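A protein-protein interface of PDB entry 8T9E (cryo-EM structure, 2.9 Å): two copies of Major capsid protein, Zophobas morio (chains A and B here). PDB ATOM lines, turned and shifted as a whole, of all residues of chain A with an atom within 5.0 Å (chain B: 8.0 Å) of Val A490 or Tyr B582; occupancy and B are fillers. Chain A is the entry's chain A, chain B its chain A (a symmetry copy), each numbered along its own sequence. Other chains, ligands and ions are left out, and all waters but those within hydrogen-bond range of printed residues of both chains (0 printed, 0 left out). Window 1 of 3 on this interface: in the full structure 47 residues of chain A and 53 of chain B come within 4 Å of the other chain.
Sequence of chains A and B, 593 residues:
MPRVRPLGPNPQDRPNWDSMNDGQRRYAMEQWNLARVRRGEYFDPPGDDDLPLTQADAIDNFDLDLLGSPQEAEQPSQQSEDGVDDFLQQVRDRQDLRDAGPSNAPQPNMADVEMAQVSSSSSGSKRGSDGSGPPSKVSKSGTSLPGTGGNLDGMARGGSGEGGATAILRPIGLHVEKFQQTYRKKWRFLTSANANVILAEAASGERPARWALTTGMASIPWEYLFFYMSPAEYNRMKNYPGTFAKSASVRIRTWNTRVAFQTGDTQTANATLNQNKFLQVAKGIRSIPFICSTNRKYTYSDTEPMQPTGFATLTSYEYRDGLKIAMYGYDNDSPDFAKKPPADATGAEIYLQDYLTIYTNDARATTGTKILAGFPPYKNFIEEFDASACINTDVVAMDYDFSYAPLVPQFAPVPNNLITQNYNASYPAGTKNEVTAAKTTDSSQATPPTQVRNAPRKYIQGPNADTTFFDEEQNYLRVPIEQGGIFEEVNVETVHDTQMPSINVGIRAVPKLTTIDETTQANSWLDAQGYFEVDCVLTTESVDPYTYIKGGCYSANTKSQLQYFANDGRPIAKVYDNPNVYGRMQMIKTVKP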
ATOM      1  N   ASN A 416      13.795 -29.139 -19.792  1.00  0.00           N
ATOM      2  CA  ASN A 416      14.237 -30.484 -20.132  1.00  0.00           C
ATOM      3  C   ASN A 416      15.594 -30.502 -20.817  1.00  0.00           C
ATOM      4  O   ASN A 416      16.143 -31.582 -21.032  1.00  0.00           O
ATOM      5  CB  ASN A 416      13.210 -31.176 -21.026  1.00  0.00           C
ATOM      6  CG  ASN A 416      12.009 -31.672 -20.255  1.00  0.00           C
ATOM      7  OD1 ASN A 416      11.984 -31.627 -19.028  1.00  0.00           O
ATOM      8  ND2 ASN A 416      11.008 -32.159 -20.975  1.00  0.00           N
ATOM      9  N   TYR A 427       8.833 -33.631 -34.001  1.00  0.00           N
ATOM     10  CA  TYR A 427       7.855 -34.704 -33.989  1.00  0.00           C
ATOM     11  C   TYR A 427       6.805 -34.390 -35.037  1.00  0.00           C
ATOM     12  O   TYR A 427       6.587 -33.217 -35.357  1.00  0.00           O
ATOM     13  CB  TYR A 427       7.209 -34.885 -32.607  1.00  0.00           C
ATOM     14  CG  TYR A 427       6.787 -33.611 -31.925  1.00  0.00           C
ATOM     15  CD1 TYR A 427       5.577 -33.010 -32.228  1.00  0.00           C
ATOM     16  CD2 TYR A 427       7.589 -33.020 -30.963  1.00  0.00           C
ATOM     17  CE1 TYR A 427       5.185 -31.852 -31.602  1.00  0.00           C
ATOM     18  CE2 TYR A 427       7.203 -31.861 -30.331  1.00  0.00           C
ATOM     19  CZ  TYR A 427       6.000 -31.283 -30.653  1.00  0.00           C
ATOM     20  OH  TYR A 427       5.603 -30.128 -30.026  1.00  0.00           O
ATOM     21  N   TYR A 459       9.319 -16.600 -25.464  1.00  0.00           N
ATOM     22  CA  TYR A 459       8.717 -17.167 -24.269  1.00  0.00           C
ATOM     23  C   TYR A 459       8.555 -16.095 -23.200  1.00  0.00           C
ATOM     24  O   TYR A 459       9.354 -15.160 -23.100  1.00  0.00           O
ATOM     25  CB  TYR A 459       9.574 -18.307 -23.729  1.00  0.00           C
ATOM     26  CG  TYR A 459       9.681 -19.497 -24.650  1.00  0.00           C
ATOM     27  CD1 TYR A 459       8.815 -20.571 -24.529  1.00  0.00           C
ATOM     28  CD2 TYR A 459      10.657 -19.552 -25.633  1.00  0.00           C
ATOM     29  CE1 TYR A 459       8.915 -21.661 -25.360  1.00  0.00           C
ATOM     30  CE2 TYR A 459      10.763 -20.640 -26.469  1.00  0.00           C
ATOM     31  CZ  TYR A 459       9.889 -21.690 -26.328  1.00  0.00           C
ATOM     32  OH  TYR A 459       9.992 -22.778 -27.158  1.00  0.00           O
ATOM     33  N   GLU A 488       0.485 -17.931 -27.228  1.00  0.00           N
ATOM     34  CA  GLU A 488       0.492 -19.291 -27.736  1.00  0.00           C
ATOM     35  C   GLU A 488       1.194 -20.186 -26.729  1.00  0.00           C
ATOM     36  O   GLU A 488       2.192 -19.800 -26.120  1.00  0.00           O
ATOM     37  CB  GLU A 488       1.180 -19.356 -29.104  1.00  0.00           C
ATOM     38  CG  GLU A 488       1.598 -20.741 -29.539  1.00  0.00           C
ATOM     39  CD  GLU A 488       2.106 -20.776 -30.965  1.00  0.00           C
ATOM     40  OE1 GLU A 488       3.161 -20.168 -31.241  1.00  0.00           O
ATOM     41  OE2 GLU A 488       1.449 -21.416 -31.808  1.00  0.00           O
ATOM     42  N   GLU A 489       0.655 -21.387 -26.552  1.00  0.00           N
ATOM     43  CA  GLU A 489       1.271 -22.403 -25.717  1.00  0.00           C
ATOM     44  C   GLU A 489       1.912 -23.464 -26.597  1.00  0.00           C
ATOM     45  O   GLU A 489       1.582 -23.602 -27.777  1.00  0.00           O
ATOM     46  CB  GLU A 489       0.257 -23.052 -24.773  1.00  0.00           C
ATOM     47  CG  GLU A 489      -0.174 -22.163 -23.633  1.00  0.00           C
ATOM     48  CD  GLU A 489      -1.201 -22.820 -22.745  1.00  0.00           C
ATOM     49  OE1 GLU A 489      -1.581 -23.973 -23.030  1.00  0.00           O
ATOM     50  OE2 GLU A 489      -1.626 -22.185 -21.757  1.00  0.00           O
ATOM     51  N   VAL A 490       2.844 -24.214 -26.014  1.00  0.00           N
ATOM     52  CA  VAL A 490       3.483 -25.296 -26.751  1.00  0.00           C
ATOM     53  C   VAL A 490       2.616 -26.532 -26.582  1.00  0.00           C
ATOM     54  O   VAL A 490       2.867 -27.369 -25.709  1.00  0.00           O
ATOM     55  CB  VAL A 490       4.923 -25.547 -26.269  1.00  0.00           C
ATOM     56  CG1 VAL A 490       5.603 -26.554 -27.174  1.00  0.00           C
ATOM     57  CG2 VAL A 490       5.699 -24.251 -26.220  1.00  0.00           C
ATOM     58  N   ASN A 491       1.590 -26.651 -27.418  1.00  0.00           N
ATOM     59  CA  ASN A 491       0.573 -27.672 -27.240  1.00  0.00           C
ATOM     60  C   ASN A 491      -0.217 -27.814 -28.530  1.00  0.00           C
ATOM     61  O   ASN A 491       0.011 -27.095 -29.505  1.00  0.00           O
ATOM     62  CB  ASN A 491      -0.360 -27.328 -26.074  1.00  0.00           C
ATOM     63  CG  ASN A 491      -0.745 -28.541 -25.263  1.00  0.00           C
ATOM     64  OD1 ASN A 491      -0.386 -29.668 -25.601  1.00  0.00           O
ATOM     65  ND2 ASN A 491      -1.477 -28.318 -24.180  1.00  0.00           N
ATOM     66  N   VAL A 492      -1.156 -28.763 -28.524  1.00  0.00           N
ATOM     67  CA  VAL A 492      -2.018 -28.981 -29.682  1.00  0.00           C
ATOM     68  C   VAL A 492      -3.336 -28.230 -29.599  1.00  0.00           C
ATOM     69  O   VAL A 492      -4.231 -28.490 -30.412  1.00  0.00           O
ATOM     70  CB  VAL A 492      -2.331 -30.476 -29.874  1.00  0.00           C
ATOM     71  CG1 VAL A 492      -1.120 -31.202 -30.419  1.00  0.00           C
ATOM     72  CG2 VAL A 492      -2.781 -31.094 -28.565  1.00  0.00           C
ATOM     73  N   ASN A 557       5.774 -28.543 -19.063  1.00  0.00           N
ATOM     74  CA  ASN A 557       6.306 -27.749 -20.162  1.00  0.00           C
ATOM     75  C   ASN A 557       5.292 -27.559 -21.282  1.00  0.00           C
ATOM     76  O   ASN A 557       5.492 -26.691 -22.136  1.00  0.00           O
ATOM     77  CB  ASN A 557       7.591 -28.385 -20.695  1.00  0.00           C
ATOM     78  CG  ASN A 557       7.393 -29.807 -21.153  1.00  0.00           C
ATOM     79  OD1 ASN A 557       6.332 -30.393 -20.954  1.00  0.00           O
ATOM     80  ND2 ASN A 557       8.422 -30.380 -21.759  1.00  0.00           N
ATOM     81  N   THR A 558       4.208 -28.337 -21.293  1.00  0.00           N
ATOM     82  CA  THR A 558       3.131 -28.096 -22.243  1.00  0.00           C
ATOM     83  C   THR A 558       2.355 -26.828 -21.922  1.00  0.00           C
ATOM     84  O   THR A 558       1.546 -26.385 -22.742  1.00  0.00           O
ATOM     85  CB  THR A 558       2.175 -29.287 -22.281  1.00  0.00           C
ATOM     86  OG1 THR A 558       1.719 -29.580 -20.956  1.00  0.00           O
ATOM     87  CG2 THR A 558       2.868 -30.504 -22.847  1.00  0.00           C
ATOM     88  N   SER A 560       3.995 -23.991 -21.261  1.00  0.00           N
ATOM     89  CA  SER A 560       4.869 -22.879 -21.611  1.00  0.00           C
ATOM     90  C   SER A 560       4.185 -21.983 -22.632  1.00  0.00           C
ATOM     91  O   SER A 560       3.564 -22.468 -23.578  1.00  0.00           O
ATOM     92  CB  SER A 560       6.191 -23.401 -22.165  1.00  0.00           C
ATOM     93  OG  SER A 560       6.970 -23.992 -21.145  1.00  0.00           O
ATOM     94  N   LEU A 562       4.091 -18.575 -25.306  1.00  0.00           N
ATOM     95  CA  LEU A 562       4.801 -17.704 -26.228  1.00  0.00           C
ATOM     96  C   LEU A 562       3.990 -16.432 -26.433  1.00  0.00           C
ATOM     97  O   LEU A 562       2.777 -16.413 -26.225  1.00  0.00           O
ATOM     98  CB  LEU A 562       5.020 -18.386 -27.581  1.00  0.00           C
ATOM     99  CG  LEU A 562       6.153 -19.387 -27.814  1.00  0.00           C
ATOM    100  CD1 LEU A 562       7.508 -18.745 -27.623  1.00  0.00           C
ATOM    101  CD2 LEU A 562       5.993 -20.614 -26.942  1.00  0.00           C
ATOM    102  N   ARG B 286       5.304 -42.779 -19.834  1.00  0.00           N
ATOM    103  CA  ARG B 286       6.177 -42.216 -20.856  1.00  0.00           C
ATOM    104  C   ARG B 286       5.590 -40.945 -21.458  1.00  0.00           C
ATOM    105  O   ARG B 286       6.332 -40.100 -21.974  1.00  0.00           O
ATOM    106  CB  ARG B 286       6.429 -43.264 -21.940  1.00  0.00           C
ATOM    107  CG  ARG B 286       7.399 -42.854 -23.019  1.00  0.00           C
ATOM    108  CD  ARG B 286       7.696 -44.015 -23.947  1.00  0.00           C
ATOM    109  NE  ARG B 286       6.501 -44.484 -24.635  1.00  0.00           N
ATOM    110  CZ  ARG B 286       6.247 -45.754 -24.913  1.00  0.00           C
ATOM    111  NH1 ARG B 286       7.098 -46.714 -24.596  1.00  0.00           N
ATOM    112  NH2 ARG B 286       5.108 -46.069 -25.522  1.00  0.00           N
ATOM    113  N   SER B 287       4.269 -40.786 -21.399  1.00  0.00           N
ATOM    114  CA  SER B 287       3.603 -39.643 -22.007  1.00  0.00           C
ATOM    115  C   SER B 287       3.577 -38.415 -21.110  1.00  0.00           C
ATOM    116  O   SER B 287       3.253 -37.325 -21.590  1.00  0.00           O
ATOM    117  CB  SER B 287       2.167 -40.010 -22.378  1.00  0.00           C
ATOM    118  OG  SER B 287       2.136 -41.024 -23.364  1.00  0.00           O
ATOM    119  N   ILE B 288       3.904 -38.561 -19.830  1.00  0.00           N
ATOM    120  CA  ILE B 288       3.770 -37.471 -18.868  1.00  0.00           C
ATOM    121  C   ILE B 288       4.830 -36.416 -19.160  1.00  0.00           C
ATOM    122  O   ILE B 288       6.028 -36.729 -19.169  1.00  0.00           O
ATOM    123  CB  ILE B 288       3.868 -37.993 -17.427  1.00  0.00           C
ATOM    124  CG1 ILE B 288       2.739 -38.986 -17.153  1.00  0.00           C
ATOM    125  CG2 ILE B 288       3.795 -36.852 -16.447  1.00  0.00           C
ATOM    126  CD1 ILE B 288       2.729 -39.524 -15.750  1.00  0.00           C
ATOM    127  N   PRO B 289       4.435 -35.167 -19.412  1.00  0.00           N
ATOM    128  CA  PRO B 289       5.407 -34.163 -19.874  1.00  0.00           C
ATOM    129  C   PRO B 289       6.526 -33.872 -18.896  1.00  0.00           C
ATOM    130  O   PRO B 289       7.661 -33.633 -19.326  1.00  0.00           O
ATOM    131  CB  PRO B 289       4.534 -32.922 -20.103  1.00  0.00           C
ATOM    132  CG  PRO B 289       3.166 -33.453 -20.300  1.00  0.00           C
ATOM    133  CD  PRO B 289       3.068 -34.627 -19.387  1.00  0.00           C
ATOM    134  N   PHE B 290       6.249 -33.876 -17.594  1.00  0.00           N
ATOM    135  CA  PHE B 290       7.217 -33.426 -16.605  1.00  0.00           C
ATOM    136  C   PHE B 290       8.009 -34.557 -15.966  1.00  0.00           C
ATOM    137  O   PHE B 290       8.872 -34.284 -15.127  1.00  0.00           O
ATOM    138  CB  PHE B 290       6.516 -32.614 -15.511  1.00  0.00           C
ATOM    139  CG  PHE B 290       5.287 -33.268 -14.962  1.00  0.00           C
ATOM    140  CD1 PHE B 290       5.371 -34.143 -13.897  1.00  0.00           C
ATOM    141  CD2 PHE B 290       4.049 -33.008 -15.512  1.00  0.00           C
ATOM    142  CE1 PHE B 290       4.242 -34.741 -13.394  1.00  0.00           C
ATOM    143  CE2 PHE B 290       2.919 -33.607 -15.011  1.00  0.00           C
ATOM    144  CZ  PHE B 290       3.017 -34.474 -13.951  1.00  0.00           C
ATOM    145  N   LYS B 439       6.739 -30.390 -36.641  1.00  0.00           N
ATOM    146  CA  LYS B 439       6.880 -29.387 -35.595  1.00  0.00           C
ATOM    147  C   LYS B 439       8.152 -29.642 -34.803  1.00  0.00           C
ATOM    148  O   LYS B 439       8.361 -30.746 -34.292  1.00  0.00           O
ATOM    149  CB  LYS B 439       5.675 -29.392 -34.656  1.00  0.00           C
ATOM    150  CG  LYS B 439       5.688 -28.251 -33.660  1.00  0.00           C
ATOM    151  CD  LYS B 439       4.536 -28.350 -32.691  1.00  0.00           C
ATOM    152  CE  LYS B 439       4.584 -27.241 -31.660  1.00  0.00           C
ATOM    153  NZ  LYS B 439       3.448 -27.337 -30.708  1.00  0.00           N
ATOM    154  N   THR B 440       8.992 -28.620 -34.702  1.00  0.00           N
ATOM    155  CA  THR B 440      10.225 -28.673 -33.933  1.00  0.00           C
ATOM    156  C   THR B 440      10.092 -27.768 -32.720  1.00  0.00           C
ATOM    157  O   THR B 440       9.785 -26.581 -32.859  1.00  0.00           O
ATOM    158  CB  THR B 440      11.421 -28.238 -34.781  1.00  0.00           C
ATOM    159  OG1 THR B 440      11.560 -29.115 -35.902  1.00  0.00           O
ATOM    160  CG2 THR B 440      12.694 -28.274 -33.959  1.00  0.00           C
ATOM    161  N   THR B 441      10.330 -28.325 -31.537  1.00  0.00           N
ATOM    162  CA  THR B 441      10.273 -27.576 -30.293  1.00  0.00           C
ATOM    163  C   THR B 441      11.644 -27.590 -29.639  1.00  0.00           C
ATOM    164  O   THR B 441      12.475 -28.453 -29.924  1.00  0.00           O
ATOM    165  CB  THR B 441       9.233 -28.151 -29.325  1.00  0.00           C
ATOM    166  OG1 THR B 441       9.327 -29.580 -29.311  1.00  0.00           O
ATOM    167  CG2 THR B 441       7.839 -27.748 -29.748  1.00  0.00           C
ATOM    168  N   ASP B 442      11.875 -26.616 -28.764  1.00  0.00           N
ATOM    169  CA  ASP B 442      13.154 -26.459 -28.077  1.00  0.00           C
ATOM    170  C   ASP B 442      12.866 -26.160 -26.610  1.00  0.00           C
ATOM    171  O   ASP B 442      12.527 -25.027 -26.259  1.00  0.00           O
ATOM    172  CB  ASP B 442      13.980 -25.353 -28.724  1.00  0.00           C
ATOM    173  CG  ASP B 442      15.370 -25.250 -28.148  1.00  0.00           C
ATOM    174  OD1 ASP B 442      15.766 -26.145 -27.381  1.00  0.00           O
ATOM    175  OD2 ASP B 442      16.075 -24.275 -28.476  1.00  0.00           O
ATOM    176  N   SER B 443      12.995 -27.175 -25.751  1.00  0.00           N
ATOM    177  CA  SER B 443      12.773 -26.965 -24.324  1.00  0.00           C
ATOM    178  C   SER B 443      13.879 -26.147 -23.679  1.00  0.00           C
ATOM    179  O   SER B 443      13.706 -25.686 -22.547  1.00  0.00           O
ATOM    180  CB  SER B 443      12.623 -28.304 -23.603  1.00  0.00           C
ATOM    181  OG  SER B 443      13.812 -29.061 -23.671  1.00  0.00           O
ATOM    182  N   SER B 444      15.008 -25.961 -24.366  1.00  0.00           N
ATOM    183  CA  SER B 444      16.000 -24.988 -23.933  1.00  0.00           C
ATOM    184  C   SER B 444      15.489 -23.562 -24.058  1.00  0.00           C
ATOM    185  O   SER B 444      16.065 -22.653 -23.452  1.00  0.00           O
ATOM    186  CB  SER B 444      17.281 -25.150 -24.747  1.00  0.00           C
ATOM    187  OG  SER B 444      18.342 -24.401 -24.189  1.00  0.00           O
ATOM    188  N   GLN B 445      14.426 -23.354 -24.837  1.00  0.00           N
ATOM    189  CA  GLN B 445      13.814 -22.052 -25.084  1.00  0.00           C
ATOM    190  C   GLN B 445      14.764 -21.080 -25.769  1.00  0.00           C
ATOM    191  O   GLN B 445      14.548 -19.867 -25.732  1.00  0.00           O
ATOM    192  CB  GLN B 445      13.265 -21.438 -23.794  1.00  0.00           C
ATOM    193  CG  GLN B 445      12.288 -22.333 -23.065  1.00  0.00           C
ATOM    194  CD  GLN B 445      11.369 -21.558 -22.161  1.00  0.00           C
ATOM    195  OE1 GLN B 445      11.587 -20.377 -21.906  1.00  0.00           O
ATOM    196  NE2 GLN B 445      10.325 -22.214 -21.678  1.00  0.00           N
ATOM    197  N   ALA B 446      15.819 -21.594 -26.402  1.00  0.00           N
ATOM    198  CA  ALA B 446      16.668 -20.740 -27.223  1.00  0.00           C
ATOM    199  C   ALA B 446      16.005 -20.415 -28.553  1.00  0.00           C
ATOM    200  O   ALA B 446      16.386 -19.444 -29.213  1.00  0.00           O
ATOM    201  CB  ALA B 446      18.021 -21.407 -27.451  1.00  0.00           C
ATOM    202  N   THR B 447      15.019 -21.213 -28.954  1.00  0.00           N
ATOM    203  CA  THR B 447      14.314 -21.071 -30.214  1.00  0.00           C
ATOM    204  C   THR B 447      12.836 -21.363 -29.995  1.00  0.00           C
ATOM    205  O   THR B 447      12.491 -22.339 -29.319  1.00  0.00           O
ATOM    206  CB  THR B 447      14.894 -22.031 -31.266  1.00  0.00           C
ATOM    207  OG1 THR B 447      16.266 -21.703 -31.509  1.00  0.00           O
ATOM    208  CG2 THR B 447      14.129 -21.940 -32.572  1.00  0.00           C
ATOM    209  N   PRO B 448      11.942 -20.538 -30.531  1.00  0.00           N
ATOM    210  CA  PRO B 448      10.509 -20.811 -30.402  1.00  0.00           C
ATOM    211  C   PRO B 448      10.119 -22.032 -31.213  1.00  0.00           C
ATOM    212  O   PRO B 448      10.813 -22.392 -32.174  1.00  0.00           O
ATOM    213  CB  PRO B 448       9.857 -19.538 -30.956  1.00  0.00           C
ATOM    214  CG  PRO B 448      10.862 -18.993 -31.891  1.00  0.00           C
ATOM    215  CD  PRO B 448      12.194 -19.292 -31.273  1.00  0.00           C
ATOM    216  N   PRO B 449       9.029 -22.706 -30.850  1.00  0.00           N
ATOM    217  CA  PRO B 449       8.569 -23.839 -31.659  1.00  0.00           C
ATOM    218  C   PRO B 449       8.230 -23.389 -33.070  1.00  0.00           C
ATOM    219  O   PRO B 449       7.723 -22.291 -33.286  1.00  0.00           O
ATOM    220  CB  PRO B 449       7.330 -24.335 -30.909  1.00  0.00           C
ATOM    221  CG  PRO B 449       6.894 -23.191 -30.084  1.00  0.00           C
ATOM    222  CD  PRO B 449       8.124 -22.428 -29.725  1.00  0.00           C
ATOM    223  N   THR B 450       8.532 -24.245 -34.036  1.00  0.00           N
ATOM    224  CA  THR B 450       8.292 -23.933 -35.436  1.00  0.00           C
ATOM    225  C   THR B 450       7.588 -25.105 -36.094  1.00  0.00           C
ATOM    226  O   THR B 450       7.667 -26.239 -35.623  1.00  0.00           O
ATOM    227  CB  THR B 450       9.590 -23.620 -36.192  1.00  0.00           C
ATOM    228  OG1 THR B 450      10.469 -24.748 -36.122  1.00  0.00           O
ATOM    229  CG2 THR B 450      10.281 -22.407 -35.599  1.00  0.00           C
ATOM    230  N   GLN B 499       0.873 -41.815 -30.420  1.00  0.00           N
ATOM    231  CA  GLN B 499       1.840 -42.499 -29.565  1.00  0.00           C
ATOM    232  C   GLN B 499       1.125 -43.598 -28.798  1.00  0.00           C
ATOM    233  O   GLN B 499       0.007 -43.391 -28.317  1.00  0.00           O
ATOM    234  CB  GLN B 499       2.529 -41.524 -28.609  1.00  0.00           C
ATOM    235  CG  GLN B 499       1.608 -40.843 -27.620  1.00  0.00           C
ATOM    236  CD  GLN B 499       2.345 -39.902 -26.700  1.00  0.00           C
ATOM    237  OE1 GLN B 499       3.541 -40.051 -26.469  1.00  0.00           O
ATOM    238  NE2 GLN B 499       1.635 -38.910 -26.181  1.00  0.00           N
ATOM    239  N   PRO B 579      13.176 -39.927 -24.089  1.00  0.00           N
ATOM    240  CA  PRO B 579      12.266 -39.135 -23.260  1.00  0.00           C
ATOM    241  C   PRO B 579      11.322 -38.309 -24.118  1.00  0.00           C
ATOM    242  O   PRO B 579      11.686 -37.824 -25.190  1.00  0.00           O
ATOM    243  CB  PRO B 579      13.211 -38.244 -22.448  1.00  0.00           C
ATOM    244  CG  PRO B 579      14.489 -38.991 -22.425  1.00  0.00           C
ATOM    245  CD  PRO B 579      14.585 -39.665 -23.756  1.00  0.00           C
ATOM    246  N   ASN B 580      10.091 -38.168 -23.641  1.00  0.00           N
ATOM    247  CA  ASN B 580       9.101 -37.395 -24.372  1.00  0.00           C
ATOM    248  C   ASN B 580       9.499 -35.925 -24.418  1.00  0.00           C
ATOM    249  O   ASN B 580      10.053 -35.376 -23.464  1.00  0.00           O
ATOM    250  CB  ASN B 580       7.717 -37.558 -23.738  1.00  0.00           C
ATOM    251  CG  ASN B 580       7.596 -36.868 -22.395  1.00  0.00           C
ATOM    252  OD1 ASN B 580       7.469 -35.650 -22.317  1.00  0.00           O
ATOM    253  ND2 ASN B 580       7.628 -37.651 -21.327  1.00  0.00           N
ATOM    254  N   VAL B 581       9.227 -35.294 -25.555  1.00  0.00           N
ATOM    255  CA  VAL B 581       9.433 -33.864 -25.732  1.00  0.00           C
ATOM    256  C   VAL B 581       8.061 -33.197 -25.736  1.00  0.00           C
ATOM    257  O   VAL B 581       7.277 -33.361 -26.679  1.00  0.00           O
ATOM    258  CB  VAL B 581      10.242 -33.552 -27.000  1.00  0.00           C
ATOM    259  CG1 VAL B 581      11.666 -34.020 -26.822  1.00  0.00           C
ATOM    260  CG2 VAL B 581       9.658 -34.257 -28.210  1.00  0.00           C
ATOM    261  N   TYR B 582       7.767 -32.464 -24.664  1.00  0.00           N
ATOM    262  CA  TYR B 582       6.468 -31.820 -24.470  1.00  0.00           C
ATOM    263  C   TYR B 582       5.330 -32.835 -24.533  1.00  0.00           C
ATOM    264  O   TYR B 582       4.255 -32.564 -25.070  1.00  0.00           O
ATOM    265  CB  TYR B 582       6.254 -30.694 -25.479  1.00  0.00           C
ATOM    266  CG  TYR B 582       7.158 -29.505 -25.265  1.00  0.00           C
ATOM    267  CD1 TYR B 582       8.404 -29.437 -25.865  1.00  0.00           C
ATOM    268  CD2 TYR B 582       6.770 -28.459 -24.451  1.00  0.00           C
ATOM    269  CE1 TYR B 582       9.230 -28.356 -25.668  1.00  0.00           C
ATOM    270  CE2 TYR B 582       7.590 -27.375 -24.247  1.00  0.00           C
ATOM    271  CZ  TYR B 582       8.817 -27.328 -24.856  1.00  0.00           C
ATOM    272  OH  TYR B 582       9.630 -26.240 -24.649  1.00  0.00           O
ATOM    273  N   GLY B 583       5.569 -34.019 -23.974  1.00  0.00           N
ATOM    274  CA  GLY B 583       4.581 -35.074 -23.971  1.00  0.00           C
ATOM    275  C   GLY B 583       4.439 -35.823 -25.274  1.00  0.00           C
ATOM    276  O   GLY B 583       3.556 -36.683 -25.382  1.00  0.00           O
ATOM    277  N   ARG B 584       5.274 -35.534 -26.265  1.00  0.00           N
ATOM    278  CA  ARG B 584       5.177 -36.152 -27.575  1.00  0.00           C
ATOM    279  C   ARG B 584       6.386 -37.032 -27.844  1.00  0.00           C
ATOM    280  O   ARG B 584       7.508 -36.722 -27.437  1.00  0.00           O
ATOM    281  CB  ARG B 584       5.072 -35.085 -28.664  1.00  0.00           C
ATOM    282  CG  ARG B 584       4.173 -33.924 -28.312  1.00  0.00           C
ATOM    283  CD  ARG B 584       2.765 -34.150 -28.805  1.00  0.00           C
ATOM    284  NE  ARG B 584       2.726 -34.247 -30.257  1.00  0.00           N
ATOM    285  CZ  ARG B 584       2.247 -33.304 -31.057  1.00  0.00           C
ATOM    286  NH1 ARG B 584       1.741 -32.182 -30.577  1.00  0.00           N
ATOM    287  NH2 ARG B 584       2.288 -33.489 -32.373  1.00  0.00           N
ATOM    288  N   MET B 585       6.146 -38.140 -28.535  1.00  0.00           N
ATOM    289  CA  MET B 585       7.236 -38.969 -29.023  1.00  0.00           C
ATOM    290  C   MET B 585       7.881 -38.302 -30.225  1.00  0.00           C
ATOM    291  O   MET B 585       7.198 -37.725 -31.074  1.00  0.00           O
ATOM    292  CB  MET B 585       6.728 -40.360 -29.398  1.00  0.00           C
ATOM    293  CG  MET B 585       6.248 -41.200 -28.225  1.00  0.00           C
ATOM    294  SD  MET B 585       7.545 -41.598 -27.039  1.00  0.00           S
ATOM    295  CE  MET B 585       7.166 -40.456 -25.723  1.00  0.00           C
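Among the printed residues, merely in contact across the chains: Val A492 with Arg B584, Asn A557 with Tyr B582, Tyr A459 with Pro B449, Asn A557 with Pro B289, Tyr A427 with Met B585, Tyr A427 with Thr B441, Tyr A427 with Arg B584, Thr A558 with Tyr B582, Tyr A459 with Gln B445, Asn A416 with Ser B443, Tyr A459 with Asp B442, Val A490 with Tyr B582, Val A490 with Thr B441, Asn A491 with Lys B439, Tyr A427 with Val B581, Tyr A459 with Pro B448, Ser A560 with Gln B445, Thr A558 with Pro B289 and Leu A562 with Pro B449.
The backbone NH (N) of Tyr A427 lies within hydrogen-bond range of the backbone carbonyl oxygen (O) of Lys B439 (2.9 Å). The backbone carbonyl oxygen (O) of Thr B447 lies within hydrogen-bond range of the side-chain hydroxyl (OH) of Tyr A459, 3.3 Å away.
The side-chain amide nitrogen (ND2) of Asn A557 sits close to the side-chain amide nitrogen (ND2) of Asn A416 (3.2 Å). O of Glu A488 is in hydrogen-bond range of N of Leu A562 (2.4 Å). The backbone NH (N) of Val A490 lies within hydrogen-bond range of the backbone carbonyl oxygen (O) of Ser A560 (3.1 Å). OD1 of Asp B442 lies close to N of Ser B444 (3.1 Å). OD2 of Asp B442 is in hydrogen-bond range of N of Ala B446. The side-chain carboxylate (OD2) of Asp B442 is in hydrogen-bond range of the backbone NH (N) of Thr B447 (3.3 Å).
Among the printed residues, no Asp or Glu carboxylate lies within 4 Å of a Lys or Arg side-chain nitrogen of the other chain.
No position is printed for both chains. Of the 21 pairs that touch across the chains among the printed residues, none has its exchanged pair printed and touching as well.
Tyr B582 touches three residues of chain A. Printed residues of chain A within 4 Å of Pro B449: Tyr A459 and Leu A562. Of the printed residues of chain B, Leu A562 touches Pro B449 (3.9 Å). Printed residues of chain B within 4 Å of Asn A416: Ser B443. Of the printed residues of chain A, Lys B439 touches Tyr A427 (2.9 Å) and Asn A491 (3.6 Å). Of the printed residues of chain B, Thr A558 touches Pro B289 and Tyr B582. The nearest residue of chain B that does not touch Val A490 is Pro B449 (4.2 Å). The nearest printed residue of chain A that does not touch Asp B442 is Val A490 (6.5 Å).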
